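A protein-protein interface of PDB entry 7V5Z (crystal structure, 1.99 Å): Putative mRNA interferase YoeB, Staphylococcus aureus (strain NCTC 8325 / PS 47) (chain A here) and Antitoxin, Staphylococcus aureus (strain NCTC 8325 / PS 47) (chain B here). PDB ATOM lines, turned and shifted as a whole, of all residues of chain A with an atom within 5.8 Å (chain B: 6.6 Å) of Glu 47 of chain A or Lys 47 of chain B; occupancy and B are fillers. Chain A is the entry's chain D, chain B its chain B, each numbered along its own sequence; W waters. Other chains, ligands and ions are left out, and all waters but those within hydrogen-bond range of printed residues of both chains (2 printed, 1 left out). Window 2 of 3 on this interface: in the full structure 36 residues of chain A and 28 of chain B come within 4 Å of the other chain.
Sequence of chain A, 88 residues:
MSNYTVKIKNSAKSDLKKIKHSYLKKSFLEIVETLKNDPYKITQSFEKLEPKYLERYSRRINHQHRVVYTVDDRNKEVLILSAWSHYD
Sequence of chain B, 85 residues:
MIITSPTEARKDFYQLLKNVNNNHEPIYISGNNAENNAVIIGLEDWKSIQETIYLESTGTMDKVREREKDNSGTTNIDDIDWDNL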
ATOM      1  N   SER A  45     -24.902 -34.869  14.149  1.00  0.00           N
ATOM      2  CA  SER A  45     -25.441 -33.859  15.072  1.00  0.00           C
ATOM      3  C   SER A  45     -24.796 -32.492  14.865  1.00  0.00           C
ATOM      4  O   SER A  45     -24.503 -31.773  15.823  1.00  0.00           O
ATOM      5  CB  SER A  45     -25.303 -34.300  16.524  1.00  0.00           C
ATOM      6  OG  SER A  45     -25.842 -35.583  16.694  1.00  0.00           O
ATOM      7  N   PHE A  46     -24.564 -32.135  13.600  1.00  0.00           N
ATOM      8  CA  PHE A  46     -24.017 -30.821  13.270  1.00  0.00           C
ATOM      9  C   PHE A  46     -24.803 -29.734  13.984  1.00  0.00           C
ATOM     10  O   PHE A  46     -26.032 -29.697  13.895  1.00  0.00           O
ATOM     11  CB  PHE A  46     -24.083 -30.599  11.762  1.00  0.00           C
ATOM     12  CG  PHE A  46     -23.771 -29.181  11.330  1.00  0.00           C
ATOM     13  CD1 PHE A  46     -22.510 -28.637  11.529  1.00  0.00           C
ATOM     14  CD2 PHE A  46     -24.732 -28.408  10.694  1.00  0.00           C
ATOM     15  CE1 PHE A  46     -22.215 -27.334  11.102  1.00  0.00           C
ATOM     16  CE2 PHE A  46     -24.450 -27.105  10.268  1.00  0.00           C
ATOM     17  CZ  PHE A  46     -23.193 -26.568  10.469  1.00  0.00           C
ATOM     18  N   GLU A  47     -24.092 -28.858  14.708  1.00  0.00           N
ATOM     19  CA  GLU A  47     -24.726 -27.772  15.451  1.00  0.00           C
ATOM     20  C   GLU A  47     -24.024 -26.458  15.146  1.00  0.00           C
ATOM     21  O   GLU A  47     -22.789 -26.390  15.164  1.00  0.00           O
ATOM     22  CB  GLU A  47     -24.693 -28.001  16.973  1.00  0.00           C
ATOM     23  CG  GLU A  47     -25.608 -29.107  17.486  1.00  0.00           C
ATOM     24  CD  GLU A  47     -27.090 -28.763  17.377  1.00  0.00           C
ATOM     25  OE1 GLU A  47     -27.449 -27.582  17.130  1.00  0.00           O
ATOM     26  OE2 GLU A  47     -27.899 -29.691  17.522  1.00  0.00           O
ATOM     27  N   LYS A  48     -24.815 -25.419  14.883  1.00  0.00           N
ATOM     28  CA  LYS A  48     -24.322 -24.047  14.837  1.00  0.00           C
ATOM     29  C   LYS A  48     -24.361 -23.494  16.255  1.00  0.00           C
ATOM     30  O   LYS A  48     -25.438 -23.289  16.817  1.00  0.00           O
ATOM     31  CB  LYS A  48     -25.176 -23.204  13.897  1.00  0.00           C
ATOM     32  CG  LYS A  48     -25.286 -23.789  12.506  1.00  0.00           C
ATOM     33  CD  LYS A  48     -25.806 -22.766  11.499  1.00  0.00           C
ATOM     34  CE  LYS A  48     -25.989 -23.430  10.135  1.00  0.00           C
ATOM     35  NZ  LYS A  48     -26.555 -22.496   9.118  1.00  0.00           N
ATOM     36  N   LEU A  49     -23.192 -23.270  16.837  1.00  0.00           N
ATOM     37  CA  LEU A  49     -23.101 -22.816  18.213  1.00  0.00           C
ATOM     38  C   LEU A  49     -23.482 -21.339  18.333  1.00  0.00           C
ATOM     39  O   LEU A  49     -23.311 -20.554  17.398  1.00  0.00           O
ATOM     40  CB  LEU A  49     -21.682 -23.038  18.726  1.00  0.00           C
ATOM     41  CG  LEU A  49     -21.146 -24.474  18.579  1.00  0.00           C
ATOM     42  CD1 LEU A  49     -19.723 -24.613  19.153  1.00  0.00           C
ATOM     43  CD2 LEU A  49     -22.102 -25.469  19.251  1.00  0.00           C
ATOM     44  N   ARG A  56     -19.075 -20.583  14.877  1.00  0.00           N
ATOM     45  CA  ARG A  56     -18.404 -21.779  15.364  1.00  0.00           C
ATOM     46  C   ARG A  56     -19.384 -22.945  15.327  1.00  0.00           C
ATOM     47  O   ARG A  56     -20.591 -22.765  15.510  1.00  0.00           O
ATOM     48  CB  ARG A  56     -17.876 -21.581  16.788  1.00  0.00           C
ATOM     49  CG  ARG A  56     -17.047 -20.334  16.958  1.00  0.00           C
ATOM     50  CD  ARG A  56     -16.024 -20.586  18.083  1.00  0.00           C
ATOM     51  NE  ARG A  56     -15.190 -19.429  18.402  1.00  0.00           N
ATOM     52  CZ  ARG A  56     -15.572 -18.437  19.197  1.00  0.00           C
ATOM     53  NH1 ARG A  56     -16.800 -18.422  19.707  1.00  0.00           N
ATOM     54  NH2 ARG A  56     -14.731 -17.450  19.463  1.00  0.00           N
ATOM     55  N   TYR A  57     -18.857 -24.147  15.095  1.00  0.00           N
ATOM     56  CA  TYR A  57     -19.694 -25.310  14.851  1.00  0.00           C
ATOM     57  C   TYR A  57     -19.229 -26.470  15.719  1.00  0.00           C
ATOM     58  O   TYR A  57     -18.083 -26.492  16.171  1.00  0.00           O
ATOM     59  CB  TYR A  57     -19.624 -25.713  13.370  1.00  0.00           C
ATOM     60  CG  TYR A  57     -19.902 -24.556  12.432  1.00  0.00           C
ATOM     61  CD1 TYR A  57     -21.210 -24.112  12.214  1.00  0.00           C
ATOM     62  CD2 TYR A  57     -18.871 -23.915  11.746  1.00  0.00           C
ATOM     63  CE1 TYR A  57     -21.476 -23.054  11.367  1.00  0.00           C
ATOM     64  CE2 TYR A  57     -19.144 -22.841  10.881  1.00  0.00           C
ATOM     65  CZ  TYR A  57     -20.451 -22.434  10.696  1.00  0.00           C
ATOM     66  OH  TYR A  57     -20.746 -21.382   9.844  1.00  0.00           O
ATOM     67  N   SER A  58     -20.117 -27.456  15.939  1.00  0.00           N
ATOM     68  CA  SER A  58     -19.675 -28.719  16.539  1.00  0.00           C
ATOM     69  C   SER A  58     -20.312 -29.916  15.841  1.00  0.00           C
ATOM     70  O   SER A  58     -21.375 -29.816  15.221  1.00  0.00           O
ATOM     71  CB  SER A  58     -19.949 -28.794  18.063  1.00  0.00           C
ATOM     72  OG  SER A  58     -21.285 -29.139  18.394  1.00  0.00           O
ATOM     73  N   ARG A  59     -19.617 -31.045  15.916  1.00  0.00           N
ATOM     74  CA  ARG A  59     -20.155 -32.339  15.530  1.00  0.00           C
ATOM     75  C   ARG A  59     -19.858 -33.323  16.651  1.00  0.00           C
ATOM     76  O   ARG A  59     -18.864 -33.180  17.369  1.00  0.00           O
ATOM     77  CB  ARG A  59     -19.552 -32.831  14.203  1.00  0.00           C
ATOM     78  CG  ARG A  59     -19.997 -32.012  13.006  1.00  0.00           C
ATOM     79  CD  ARG A  59     -19.223 -32.353  11.730  1.00  0.00           C
ATOM     80  NE  ARG A  59     -19.782 -31.498  10.714  1.00  0.00           N
ATOM     81  CZ  ARG A  59     -20.816 -31.821   9.950  1.00  0.00           C
ATOM     82  NH1 ARG A  59     -21.357 -33.039  10.021  1.00  0.00           N
ATOM     83  NH2 ARG A  59     -21.289 -30.927   9.103  1.00  0.00           N
ATOM     84  N   GLY B  42     -38.195 -22.937  17.874  1.00  0.00           N
ATOM     85  CA  GLY B  42     -37.941 -24.053  16.980  1.00  0.00           C
ATOM     86  C   GLY B  42     -36.917 -25.013  17.565  1.00  0.00           C
ATOM     87  O   GLY B  42     -36.019 -24.621  18.303  1.00  0.00           O
ATOM     88  N   LEU B  43     -37.063 -26.294  17.231  1.00  0.00           N
ATOM     89  CA  LEU B  43     -36.223 -27.303  17.872  1.00  0.00           C
ATOM     90  C   LEU B  43     -34.757 -27.127  17.491  1.00  0.00           C
ATOM     91  O   LEU B  43     -33.865 -27.302  18.328  1.00  0.00           O
ATOM     92  CB  LEU B  43     -36.714 -28.710  17.511  1.00  0.00           C
ATOM     93  CG  LEU B  43     -35.813 -29.854  17.998  1.00  0.00           C
ATOM     94  CD1 LEU B  43     -35.829 -29.942  19.532  1.00  0.00           C
ATOM     95  CD2 LEU B  43     -36.210 -31.189  17.375  1.00  0.00           C
ATOM     96  N   GLU B  44     -34.478 -26.773  16.239  1.00  0.00           N
ATOM     97  CA  GLU B  44     -33.082 -26.609  15.850  1.00  0.00           C
ATOM     98  C   GLU B  44     -32.412 -25.508  16.659  1.00  0.00           C
ATOM     99  O   GLU B  44     -31.269 -25.664  17.102  1.00  0.00           O
ATOM    100  CB  GLU B  44     -32.983 -26.330  14.357  1.00  0.00           C
ATOM    101  CG  GLU B  44     -33.150 -27.598  13.546  1.00  0.00           C
ATOM    102  CD  GLU B  44     -33.167 -27.356  12.049  1.00  0.00           C
ATOM    103  OE1 GLU B  44     -33.836 -28.152  11.349  1.00  0.00           O
ATOM    104  OE2 GLU B  44     -32.515 -26.388  11.583  1.00  0.00           O
ATOM    105  N   ASP B  45     -33.120 -24.401  16.894  1.00  0.00           N
ATOM    106  CA  ASP B  45     -32.540 -23.312  17.671  1.00  0.00           C
ATOM    107  C   ASP B  45     -32.382 -23.703  19.131  1.00  0.00           C
ATOM    108  O   ASP B  45     -31.408 -23.307  19.783  1.00  0.00           O
ATOM    109  CB  ASP B  45     -33.398 -22.049  17.547  1.00  0.00           C
ATOM    110  CG  ASP B  45     -33.332 -21.434  16.159  1.00  0.00           C
ATOM    111  OD1 ASP B  45     -32.352 -21.708  15.435  1.00  0.00           O
ATOM    112  OD2 ASP B  45     -34.247 -20.659  15.798  1.00  0.00           O
ATOM    113  N   TRP B  46     -33.345 -24.454  19.663  1.00  0.00           N
ATOM    114  CA  TRP B  46     -33.229 -24.983  21.019  1.00  0.00           C
ATOM    115  C   TRP B  46     -32.016 -25.897  21.144  1.00  0.00           C
ATOM    116  O   TRP B  46     -31.246 -25.800  22.109  1.00  0.00           O
ATOM    117  CB  TRP B  46     -34.508 -25.733  21.397  1.00  0.00           C
ATOM    118  CG  TRP B  46     -34.444 -26.454  22.735  1.00  0.00           C
ATOM    119  CD1 TRP B  46     -34.246 -27.795  22.943  1.00  0.00           C
ATOM    120  CD2 TRP B  46     -34.608 -25.869  24.037  1.00  0.00           C
ATOM    121  NE1 TRP B  46     -34.265 -28.071  24.296  1.00  0.00           N
ATOM    122  CE2 TRP B  46     -34.493 -26.906  24.983  1.00  0.00           C
ATOM    123  CE3 TRP B  46     -34.829 -24.567  24.491  1.00  0.00           C
ATOM    124  CZ2 TRP B  46     -34.591 -26.679  26.355  1.00  0.00           C
ATOM    125  CZ3 TRP B  46     -34.934 -24.346  25.864  1.00  0.00           C
ATOM    126  CH2 TRP B  46     -34.814 -25.396  26.772  1.00  0.00           C
ATOM    127  N   LYS B  47     -31.806 -26.759  20.150  1.00  0.00           N
ATOM    128  CA  LYS B  47     -30.661 -27.660  20.184  1.00  0.00           C
ATOM    129  C   LYS B  47     -29.345 -26.892  20.129  1.00  0.00           C
ATOM    130  O   LYS B  47     -28.381 -27.268  20.813  1.00  0.00           O
ATOM    131  CB  LYS B  47     -30.751 -28.662  19.037  1.00  0.00           C
ATOM    132  CG  LYS B  47     -31.809 -29.758  19.234  1.00  0.00           C
ATOM    133  CD  LYS B  47     -31.714 -30.763  18.090  1.00  0.00           C
ATOM    134  CE  LYS B  47     -32.559 -32.000  18.338  1.00  0.00           C
ATOM    135  NZ  LYS B  47     -32.552 -32.916  17.146  1.00  0.00           N
ATOM    136  N   SER B  48     -29.278 -25.830  19.312  1.00  0.00           N
ATOM    137  CA  SER B  48     -28.094 -24.972  19.300  1.00  0.00           C
ATOM    138  C   SER B  48     -27.832 -24.396  20.677  1.00  0.00           C
ATOM    139  O   SER B  48     -26.684 -24.331  21.134  1.00  0.00           O
ATOM    140  CB  SER B  48     -28.256 -23.811  18.306  1.00  0.00           C
ATOM    141  OG  SER B  48     -28.021 -24.215  16.977  1.00  0.00           O
ATOM    142  N   ILE B  49     -28.877 -23.881  21.318  1.00  0.00           N
ATOM    143  CA  ILE B  49     -28.696 -23.279  22.627  1.00  0.00           C
ATOM    144  C   ILE B  49     -28.193 -24.320  23.617  1.00  0.00           C
ATOM    145  O   ILE B  49     -27.248 -24.081  24.379  1.00  0.00           O
ATOM    146  CB  ILE B  49     -30.009 -22.636  23.103  1.00  0.00           C
ATOM    147  CG1 ILE B  49     -30.308 -21.360  22.297  1.00  0.00           C
ATOM    148  CG2 ILE B  49     -29.960 -22.399  24.596  1.00  0.00           C
ATOM    149  CD1 ILE B  49     -31.715 -20.806  22.539  1.00  0.00           C
ATOM    150  N   GLN B  50     -28.839 -25.489  23.637  1.00  0.00           N
ATOM    151  CA  GLN B  50     -28.472 -26.490  24.628  1.00  0.00           C
ATOM    152  C   GLN B  50     -27.055 -26.977  24.385  1.00  0.00           C
ATOM    153  O   GLN B  50     -26.285 -27.170  25.331  1.00  0.00           O
ATOM    154  CB  GLN B  50     -29.469 -27.652  24.603  1.00  0.00           C
ATOM    155  CG  GLN B  50     -30.865 -27.268  25.115  1.00  0.00           C
ATOM    156  CD  GLN B  50     -30.839 -26.732  26.552  1.00  0.00           C
ATOM    157  OE1 GLN B  50     -30.130 -27.262  27.407  1.00  0.00           O
ATOM    158  NE2 GLN B  50     -31.613 -25.683  26.816  1.00  0.00           N
ATOM    159  N   GLU B  51     -26.685 -27.156  23.118  1.00  0.00           N
ATOM    160  CA  GLU B  51     -25.325 -27.592  22.818  1.00  0.00           C
ATOM    161  C   GLU B  51     -24.310 -26.531  23.228  1.00  0.00           C
ATOM    162  O   GLU B  51     -23.208 -26.861  23.683  1.00  0.00           O
ATOM    163  CB  GLU B  51     -25.196 -27.938  21.335  1.00  0.00           C
ATOM    164  CG  GLU B  51     -23.776 -28.159  20.859  1.00  0.00           C
ATOM    165  CD  GLU B  51     -23.270 -29.567  21.155  1.00  0.00           C
ATOM    166  OE1 GLU B  51     -24.004 -30.360  21.795  1.00  0.00           O
ATOM    167  OE2 GLU B  51     -22.137 -29.873  20.743  1.00  0.00           O
ATOM    168  N   THR B  52     -24.667 -25.253  23.093  1.00  0.00           N
ATOM    169  CA  THR B  52     -23.755 -24.192  23.512  1.00  0.00           C
ATOM    170  C   THR B  52     -23.558 -24.199  25.019  1.00  0.00           C
ATOM    171  O   THR B  52     -22.428 -24.085  25.511  1.00  0.00           O
ATOM    172  CB  THR B  52     -24.277 -22.821  23.058  1.00  0.00           C
ATOM    173  OG1 THR B  52     -24.352 -22.799  21.637  1.00  0.00           O
ATOM    174  CG2 THR B  52     -23.308 -21.721  23.499  1.00  0.00           C
HETATM  175  O   HOH W   1     -22.714 -31.493  17.902  1.00  0.00           O
HETATM  176  O   HOH W   2     -29.780 -27.900  15.705  1.00  0.00           O
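The side-chain carboxylate (OE1) of Glu 47 of chain A sits at hydrogen-bond distance from the backbone NH (N) of Ser 48 of chain B, at 3.3 Å. OG of Ser 48 of chain B is in hydrogen-bond range of O of Lys 48 of chain A, 2.7 Å away. The side-chain carboxylate (OE2) of Glu 51 of chain B sits at hydrogen-bond distance from the side-chain hydroxyl (OG) of Ser 58 of chain A (2.6 Å).
The backbone carbonyl oxygen (O) of Ser 48 of chain B is in hydrogen-bond range of the side-chain hydroxyl (OG1) of Thr 52 of chain B, at 2.8 Å. O of Ser 58 of chain A sits at hydrogen-bond distance from N of Glu 47 of chain A, 2.9 Å away. N of Leu 49 of chain A lies within hydrogen-bond range of O of Arg 56 of chain A, 3.0 Å away.
Glu 47 of chain A touches Lys 47 of chain B. CG of Glu 47 of chain A touches CG of Glu 51 of chain B (3.95 Å). Leu 49 of chain A touches Glu 51 of chain B (CD2 to CG, 3.6 Å). Leu 49 of chain A touches Thr 52 of chain B.
Glu 47 of chain A touches just these residues of chain B: Lys 47, Ser 48 and Glu 51. Of chain A, only Glu 47 (3.4 Å) comes within 4 Å of Lys 47 of chain B. Of the printed residues of chain A, Glu 51 of chain B touches Glu 47 (3.95 Å), Leu 49 (3.6 Å) and Ser 58 (2.6 Å). Printed residues of chain B within 4 Å of Ser 58 of chain A: Glu 51. Printed residues of chain A within 4 Å of Thr 52 of chain B: Leu 49 (3.6 Å). Of the printed residues of chain A, Ser 48 of chain B touches Glu 47 and Lys 48. The nearest residue of chain B that does not touch Glu 47 of chain A is Glu 44 of chain B (4.3 Å). The nearest printed residue of chain B that does not touch Ser 58 of chain A is Thr 52 of chain B (7.0 Å).
Hydrophobic or aromatic side chains of chain A within 4 Å of the printed part of chain B: Leu 49. Among the printed residues, no Asp or Glu carboxylate lies within 4 Å of a Lys or Arg side-chain nitrogen of the other chain.
Water W2 bridges the side-chain carboxylate of Glu 47 of chain A and the backbone carbonyl oxygen of Glu 44 of chain B. Water W1 lies within hydrogen-bond range of the backbone carbonyl oxygen of Ser 45 of chain A, the side-chain hydroxyl of Ser 58 of chain A and the side-chain carboxylate of Glu 51 of chain B.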
